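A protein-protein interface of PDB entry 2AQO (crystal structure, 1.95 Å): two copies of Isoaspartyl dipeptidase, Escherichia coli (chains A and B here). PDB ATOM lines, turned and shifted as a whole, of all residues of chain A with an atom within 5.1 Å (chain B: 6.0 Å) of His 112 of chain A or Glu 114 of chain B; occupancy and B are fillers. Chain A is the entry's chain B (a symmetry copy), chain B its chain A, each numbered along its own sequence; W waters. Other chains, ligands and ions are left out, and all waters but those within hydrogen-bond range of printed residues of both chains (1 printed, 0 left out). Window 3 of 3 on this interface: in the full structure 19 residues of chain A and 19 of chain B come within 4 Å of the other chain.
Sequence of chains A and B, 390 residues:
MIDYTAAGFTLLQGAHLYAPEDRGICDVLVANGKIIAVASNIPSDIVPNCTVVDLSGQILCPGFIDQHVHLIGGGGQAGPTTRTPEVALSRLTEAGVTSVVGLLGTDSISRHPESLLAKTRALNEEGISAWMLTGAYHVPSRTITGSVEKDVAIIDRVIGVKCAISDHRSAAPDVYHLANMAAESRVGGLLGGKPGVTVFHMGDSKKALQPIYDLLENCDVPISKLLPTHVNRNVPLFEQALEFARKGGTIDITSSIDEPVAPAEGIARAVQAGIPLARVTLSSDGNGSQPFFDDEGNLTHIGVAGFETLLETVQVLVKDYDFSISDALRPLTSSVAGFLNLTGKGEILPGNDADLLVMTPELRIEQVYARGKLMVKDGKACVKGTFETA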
ATOM      1  N   ILE A  72      33.877  14.071  20.829  1.00  0.00           N
ATOM      2  CA  ILE A  72      32.795  13.768  19.881  1.00  0.00           C
ATOM      3  C   ILE A  72      31.457  14.403  20.250  1.00  0.00           C
ATOM      4  O   ILE A  72      30.455  14.248  19.536  1.00  0.00           O
ATOM      5  CB  ILE A  72      32.649  12.266  19.617  1.00  0.00           C
ATOM      6  CG1 ILE A  72      32.474  11.448  20.901  1.00  0.00           C
ATOM      7  CG2 ILE A  72      33.839  11.791  18.775  1.00  0.00           C
ATOM      8  CD1 ILE A  72      31.788  10.082  20.638  1.00  0.00           C
ATOM      9  N   LEU A 104      34.728  10.001  27.146  1.00  0.00           N
ATOM     10  CA  LEU A 104      33.268   9.939  27.189  1.00  0.00           C
ATOM     11  C   LEU A 104      32.826  10.249  28.637  1.00  0.00           C
ATOM     12  O   LEU A 104      33.631  10.178  29.585  1.00  0.00           O
ATOM     13  CB  LEU A 104      32.756   8.539  26.779  1.00  0.00           C
ATOM     14  CG  LEU A 104      33.182   8.177  25.344  1.00  0.00           C
ATOM     15  CD1 LEU A 104      32.544   6.820  25.003  1.00  0.00           C
ATOM     16  CD2 LEU A 104      32.740   9.275  24.346  1.00  0.00           C
ATOM     17  N   ILE A 109      25.799   5.014  25.597  1.00  0.00           N
ATOM     18  CA  ILE A 109      24.789   4.268  24.822  1.00  0.00           C
ATOM     19  C   ILE A 109      24.775   4.888  23.426  1.00  0.00           C
ATOM     20  O   ILE A 109      24.896   4.211  22.406  1.00  0.00           O
ATOM     21  CB  ILE A 109      23.407   4.427  25.459  1.00  0.00           C
ATOM     22  CG1 ILE A 109      23.407   3.869  26.873  1.00  0.00           C
ATOM     23  CG2 ILE A 109      22.320   3.730  24.631  1.00  0.00           C
ATOM     24  CD1 ILE A 109      23.220   2.368  26.936  1.00  0.00           C
ATOM     25  N   SER A 110      24.634   6.232  23.386  1.00  0.00           N
ATOM     26  CA  SER A 110      24.651   6.863  22.061  1.00  0.00           C
ATOM     27  C   SER A 110      26.069   7.295  21.715  1.00  0.00           C
ATOM     28  O   SER A 110      26.254   7.782  20.615  1.00  0.00           O
ATOM     29  CB  SER A 110      23.761   8.085  21.961  1.00  0.00           C
ATOM     30  OG  SER A 110      24.439   9.202  22.578  1.00  0.00           O
ATOM     31  N   ARG A 111      27.028   7.117  22.642  1.00  0.00           N
ATOM     32  CA  ARG A 111      28.420   7.499  22.429  1.00  0.00           C
ATOM     33  C   ARG A 111      29.287   6.263  22.503  1.00  0.00           C
ATOM     34  O   ARG A 111      29.116   5.530  23.444  1.00  0.00           O
ATOM     35  CB  ARG A 111      28.905   8.543  23.430  1.00  0.00           C
ATOM     36  CG  ARG A 111      27.940   9.732  23.468  1.00  0.00           C
ATOM     37  CD  ARG A 111      27.876  10.515  22.157  1.00  0.00           C
ATOM     38  NE  ARG A 111      27.334  11.868  22.414  1.00  0.00           N
ATOM     39  CZ  ARG A 111      27.271  12.879  21.560  1.00  0.00           C
ATOM     40  NH1 ARG A 111      27.702  12.749  20.312  1.00  0.00           N
ATOM     41  NH2 ARG A 111      26.772  14.073  21.963  1.00  0.00           N
ATOM     42  N   HIS A 112      30.198   6.073  21.525  1.00  0.00           N
ATOM     43  CA  HIS A 112      31.059   4.907  21.441  1.00  0.00           C
ATOM     44  C   HIS A 112      32.583   5.173  21.370  1.00  0.00           C
ATOM     45  O   HIS A 112      33.044   6.079  20.698  1.00  0.00           O
ATOM     46  CB  HIS A 112      30.616   4.016  20.236  1.00  0.00           C
ATOM     47  CG  HIS A 112      29.137   3.747  20.257  1.00  0.00           C
ATOM     48  ND1 HIS A 112      28.201   4.699  19.845  1.00  0.00           N
ATOM     49  CD2 HIS A 112      28.454   2.651  20.703  1.00  0.00           C
ATOM     50  CE1 HIS A 112      26.981   4.161  20.005  1.00  0.00           C
ATOM     51  NE2 HIS A 112      27.107   2.947  20.544  1.00  0.00           N
ATOM     52  N   PRO A 113      33.390   4.325  22.009  1.00  0.00           N
ATOM     53  CA  PRO A 113      34.847   4.527  21.963  1.00  0.00           C
ATOM     54  C   PRO A 113      35.381   4.478  20.550  1.00  0.00           C
ATOM     55  O   PRO A 113      36.314   5.168  20.216  1.00  0.00           O
ATOM     56  CB  PRO A 113      35.484   3.452  22.853  1.00  0.00           C
ATOM     57  CG  PRO A 113      34.364   2.596  23.397  1.00  0.00           C
ATOM     58  CD  PRO A 113      33.042   3.149  22.852  1.00  0.00           C
ATOM     59  N   GLU A 114      34.768   3.676  19.683  1.00  0.00           N
ATOM     60  CA  GLU A 114      35.201   3.641  18.312  1.00  0.00           C
ATOM     61  C   GLU A 114      35.008   4.953  17.604  1.00  0.00           C
ATOM     62  O   GLU A 114      35.818   5.306  16.746  1.00  0.00           O
ATOM     63  CB  GLU A 114      34.476   2.590  17.499  1.00  0.00           C
ATOM     64  CG  GLU A 114      34.822   1.201  18.038  1.00  0.00           C
ATOM     65  CD  GLU A 114      33.865   0.747  19.088  1.00  0.00           C
ATOM     66  OE1 GLU A 114      33.101   1.488  19.679  1.00  0.00           O
ATOM     67  OE2 GLU A 114      34.017  -0.518  19.326  1.00  0.00           O
ATOM     68  N   SER A 115      33.919   5.641  17.915  1.00  0.00           N
ATOM     69  CA  SER A 115      33.697   6.961  17.321  1.00  0.00           C
ATOM     70  C   SER A 115      34.745   7.949  17.857  1.00  0.00           C
ATOM     71  O   SER A 115      35.313   8.777  17.145  1.00  0.00           O
ATOM     72  CB  SER A 115      32.337   7.509  17.711  1.00  0.00           C
ATOM     73  OG  SER A 115      31.310   6.570  17.388  1.00  0.00           O
ATOM     74  N   LEU A 116      34.987   7.869  19.161  1.00  0.00           N
ATOM     75  CA  LEU A 116      35.942   8.738  19.823  1.00  0.00           C
ATOM     76  C   LEU A 116      37.352   8.534  19.269  1.00  0.00           C
ATOM     77  O   LEU A 116      38.128   9.479  19.037  1.00  0.00           O
ATOM     78  CB  LEU A 116      35.869   8.562  21.365  1.00  0.00           C
ATOM     79  CG  LEU A 116      36.942   9.349  22.126  1.00  0.00           C
ATOM     80  CD1 LEU A 116      36.767  10.880  21.983  1.00  0.00           C
ATOM     81  CD2 LEU A 116      36.906   8.982  23.605  1.00  0.00           C
ATOM     82  N   LEU A 117      37.661   7.273  19.035  1.00  0.00           N
ATOM     83  CA  LEU A 117      38.947   6.911  18.455  1.00  0.00           C
ATOM     84  C   LEU A 117      39.133   7.518  17.035  1.00  0.00           C
ATOM     85  O   LEU A 117      40.234   7.953  16.645  1.00  0.00           O
ATOM     86  CB  LEU A 117      39.145   5.370  18.419  1.00  0.00           C
ATOM     87  CG  LEU A 117      40.410   4.964  17.619  1.00  0.00           C
ATOM     88  CD1 LEU A 117      41.665   5.462  18.338  1.00  0.00           C
ATOM     89  CD2 LEU A 117      40.492   3.426  17.495  1.00  0.00           C
ATOM     90  N   HIS B 112      27.039   4.257  14.587  1.00  0.00           N
ATOM     91  CA  HIS B 112      26.195   3.270  15.225  1.00  0.00           C
ATOM     92  C   HIS B 112      24.716   3.621  15.160  1.00  0.00           C
ATOM     93  O   HIS B 112      24.342   4.781  15.305  1.00  0.00           O
ATOM     94  CB  HIS B 112      26.627   3.212  16.712  1.00  0.00           C
ATOM     95  CG  HIS B 112      28.132   3.055  16.835  1.00  0.00           C
ATOM     96  ND1 HIS B 112      28.729   1.851  17.212  1.00  0.00           N
ATOM     97  CD2 HIS B 112      29.150   3.938  16.608  1.00  0.00           C
ATOM     98  CE1 HIS B 112      30.061   2.012  17.227  1.00  0.00           C
ATOM     99  NE2 HIS B 112      30.336   3.267  16.861  1.00  0.00           N
ATOM    100  N   PRO B 113      23.866   2.584  14.996  1.00  0.00           N
ATOM    101  CA  PRO B 113      22.425   2.806  14.936  1.00  0.00           C
ATOM    102  C   PRO B 113      21.870   3.470  16.205  1.00  0.00           C
ATOM    103  O   PRO B 113      20.865   4.191  16.172  1.00  0.00           O
ATOM    104  CB  PRO B 113      21.761   1.410  14.746  1.00  0.00           C
ATOM    105  CG  PRO B 113      22.858   0.357  14.855  1.00  0.00           C
ATOM    106  CD  PRO B 113      24.178   1.125  14.877  1.00  0.00           C
ATOM    107  N   GLU B 114      22.513   3.207  17.356  1.00  0.00           N
ATOM    108  CA  GLU B 114      22.032   3.812  18.596  1.00  0.00           C
ATOM    109  C   GLU B 114      22.217   5.313  18.563  1.00  0.00           C
ATOM    110  O   GLU B 114      21.388   6.053  19.088  1.00  0.00           O
ATOM    111  CB  GLU B 114      22.753   3.211  19.823  1.00  0.00           C
ATOM    112  CG  GLU B 114      22.404   1.723  20.005  1.00  0.00           C
ATOM    113  CD  GLU B 114      23.368   0.821  19.279  1.00  0.00           C
ATOM    114  OE1 GLU B 114      24.203   1.256  18.489  1.00  0.00           O
ATOM    115  OE2 GLU B 114      23.182  -0.471  19.585  1.00  0.00           O
ATOM    116  N   SER B 115      23.318   5.745  17.944  1.00  0.00           N
ATOM    117  CA  SER B 115      23.557   7.180  17.830  1.00  0.00           C
ATOM    118  C   SER B 115      22.493   7.782  16.930  1.00  0.00           C
ATOM    119  O   SER B 115      21.861   8.761  17.256  1.00  0.00           O
ATOM    120  CB  SER B 115      24.925   7.417  17.260  1.00  0.00           C
ATOM    121  OG  SER B 115      25.921   6.741  18.032  1.00  0.00           O
ATOM    122  N   LEU B 116      22.288   7.128  15.779  1.00  0.00           N
ATOM    123  CA  LEU B 116      21.300   7.552  14.831  1.00  0.00           C
ATOM    124  C   LEU B 116      19.935   7.608  15.501  1.00  0.00           C
ATOM    125  O   LEU B 116      19.156   8.554  15.298  1.00  0.00           O
ATOM    126  CB  LEU B 116      21.302   6.594  13.612  1.00  0.00           C
ATOM    127  CG  LEU B 116      20.257   6.984  12.523  1.00  0.00           C
ATOM    128  CD1 LEU B 116      20.487   8.428  12.034  1.00  0.00           C
ATOM    129  CD2 LEU B 116      20.408   6.037  11.339  1.00  0.00           C
ATOM    130  N   LEU B 117      19.614   6.591  16.294  1.00  0.00           N
ATOM    131  CA  LEU B 117      18.324   6.607  16.961  1.00  0.00           C
ATOM    132  C   LEU B 117      18.136   7.799  17.888  1.00  0.00           C
ATOM    133  O   LEU B 117      17.062   8.442  17.928  1.00  0.00           O
ATOM    134  CB  LEU B 117      18.026   5.261  17.630  1.00  0.00           C
ATOM    135  CG  LEU B 117      16.785   5.257  18.526  1.00  0.00           C
ATOM    136  CD1 LEU B 117      15.494   5.230  17.700  1.00  0.00           C
ATOM    137  CD2 LEU B 117      16.830   3.987  19.389  1.00  0.00           C
ATOM    138  N   ALA B 118      19.168   8.130  18.661  1.00  0.00           N
ATOM    139  CA  ALA B 118      19.072   9.263  19.579  1.00  0.00           C
ATOM    140  C   ALA B 118      18.819  10.564  18.819  1.00  0.00           C
ATOM    141  O   ALA B 118      17.963  11.369  19.191  1.00  0.00           O
ATOM    142  CB  ALA B 118      20.355   9.417  20.405  1.00  0.00           C
ATOM    143  N   LYS B 119      19.566  10.748  17.726  1.00  0.00           N
ATOM    144  CA  LYS B 119      19.449  11.946  16.883  1.00  0.00           C
ATOM    145  C   LYS B 119      18.048  12.062  16.294  1.00  0.00           C
ATOM    146  O   LYS B 119      17.457  13.146  16.213  1.00  0.00           O
ATOM    147  CB  LYS B 119      20.502  11.881  15.793  1.00  0.00           C
ATOM    148  CG  LYS B 119      20.464  13.064  14.827  1.00  0.00           C
ATOM    149  CD  LYS B 119      20.689  14.425  15.487  1.00  0.00           C
ATOM    150  CE  LYS B 119      20.792  15.549  14.443  1.00  0.00           C
ATOM    151  NZ  LYS B 119      21.312  16.772  15.077  1.00  0.00           N
ATOM    152  N   MET B 132      14.044   6.191  11.030  1.00  0.00           N
ATOM    153  CA  MET B 132      15.346   5.765  10.551  1.00  0.00           C
ATOM    154  C   MET B 132      15.258   4.378   9.999  1.00  0.00           C
ATOM    155  O   MET B 132      14.242   3.678  10.167  1.00  0.00           O
ATOM    156  CB  MET B 132      16.401   5.803  11.682  1.00  0.00           C
ATOM    157  CG  MET B 132      16.029   4.831  12.805  1.00  0.00           C
ATOM    158  SD  MET B 132      17.206   4.678  14.197  1.00  0.00           S
ATOM    159  CE  MET B 132      18.338   3.415  13.557  1.00  0.00           C
ATOM    160  N   THR B 143      22.910  -4.205  13.746  1.00  0.00           N
ATOM    161  CA  THR B 143      21.660  -3.679  14.270  1.00  0.00           C
ATOM    162  C   THR B 143      21.751  -3.294  15.716  1.00  0.00           C
ATOM    163  O   THR B 143      22.767  -3.401  16.393  1.00  0.00           O
ATOM    164  CB  THR B 143      20.551  -4.743  14.094  1.00  0.00           C
ATOM    165  OG1 THR B 143      20.999  -5.920  14.733  1.00  0.00           O
ATOM    166  CG2 THR B 143      20.330  -5.080  12.627  1.00  0.00           C
ATOM    167  N   ILE B 144      20.615  -2.866  16.195  1.00  0.00           N
ATOM    168  CA  ILE B 144      20.510  -2.497  17.598  1.00  0.00           C
ATOM    169  C   ILE B 144      20.202  -3.697  18.480  1.00  0.00           C
ATOM    170  O   ILE B 144      20.847  -3.915  19.505  1.00  0.00           O
ATOM    171  CB  ILE B 144      19.406  -1.457  17.788  1.00  0.00           C
ATOM    172  CG1 ILE B 144      19.753  -0.193  16.997  1.00  0.00           C
ATOM    173  CG2 ILE B 144      19.147  -1.172  19.264  1.00  0.00           C
ATOM    174  CD1 ILE B 144      18.654   0.854  17.086  1.00  0.00           C
ATOM    175  N   THR B 145      19.205  -4.480  18.102  1.00  0.00           N
ATOM    176  CA  THR B 145      18.823  -5.591  18.984  1.00  0.00           C
ATOM    177  C   THR B 145      19.488  -6.897  18.654  1.00  0.00           C
ATOM    178  O   THR B 145      19.274  -7.871  19.376  1.00  0.00           O
ATOM    179  CB  THR B 145      17.308  -5.848  18.949  1.00  0.00           C
ATOM    180  OG1 THR B 145      16.963  -6.316  17.617  1.00  0.00           O
ATOM    181  CG2 THR B 145      16.577  -4.576  19.348  1.00  0.00           C
HETATM  182  O   HOH W   1      29.209   7.217  19.073  1.00  0.00           O
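OG of Ser 115 of chain A lies within hydrogen-bond range of NE2 of His 112 of chain B, 3.5 Å away.
OG of Ser 115 of chain B lies within hydrogen-bond range of O of Ser 110 of chain A (2.8 Å).
Water W1 lies within hydrogen-bond range of the side-chain hydroxyl (OG) of Ser 115 of chain A (2.8 Å), a ring nitrogen (ND1) of His 112 of chain A (2.8 Å), the backbone carbonyl oxygen (O) of Ser 110 of chain A (3.4 Å) and the side-chain hydroxyl (OG) of Ser 115 of chain B (3.5 Å).
Hydrophobic or aromatic side chains of chain B that line the printed part of chain A: His 112 and Ala 118.
Of the 11 printed residues of chain A, 5 touch a printed residue of chain B.
Printed residues of chain A that touch a printed residue of chain B: Ile 109, Ser 110, His 112, Glu 114 and Ser 115.
Hydrophobic or aromatic side chains of chain A within 4 Å of the printed part of chain B: His 112.
Among the printed residues, no Asp or Glu carboxylate lies within 4 Å of a Lys or Arg side-chain nitrogen of the other chain.
Among the printed residues, merely in contact across the chains: Ile 109 of chain A with Glu 114 of chain B, Ser 110 of chain A with Ala 118 of chain B, His 112 of chain A with His 112 of chain B, His 112 of chain A with Glu 114 of chain B, His 112 of chain A with Ser 115 of chain B and Glu 114 of chain A with His 112 of chain B.
His 112 of chain B touches its own counterpart, His 112 of chain A.
His 112 of chain A touches Glu 114 of chain B, and with the chains exchanged Glu 114 of chain A touches His 112 of chain B.
His 112 of chain A touches Ser 115 of chain B, and with the chains exchanged Ser 115 of chain A touches His 112 of chain B.
Positions printed for both chains: 112, 113, 114, 115, 116 and 117.
Of the 8 pairs that touch across the chains among the printed residues, 5 have their exchanged pair printed and touching as well.
The backbone carbonyl oxygen (O) of Ile 109 of chain A lies within hydrogen-bond range of a ring nitrogen (NE2) of His 112 of chain A (3.2 Å).
Of the printed residues of chain B, Glu 114 of chain A touches His 112 (3.9 Å).
Printed residues of chain B within 4 Å of Ser 115 of chain A: His 112.
Printed residues of chain A within 4 Å of His 112 of chain B: His 112 (3.4 Å), Glu 114 (3.9 Å) and Ser 115 (3.5 Å).
Glu 114 of chain B touches just these residues of chain A: Ile 109 (3.5 Å) and His 112 (3.9 Å).
Of the printed residues of chain A, Ser 115 of chain B touches Ser 110 and His 112.
Printed residues of chain A within 4 Å of Ala 118 of chain B: Ser 110 (3.97 Å).
Thr 145 of chain B touches none of the printed residues of chain A.
The nearest printed residue of chain B that does not touch His 112 of chain A is Pro 113 of chain B (6.1 Å).
The nearest residue of chain A that does not touch Glu 114 of chain B is Ser 110 of chain A (4.2 Å).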
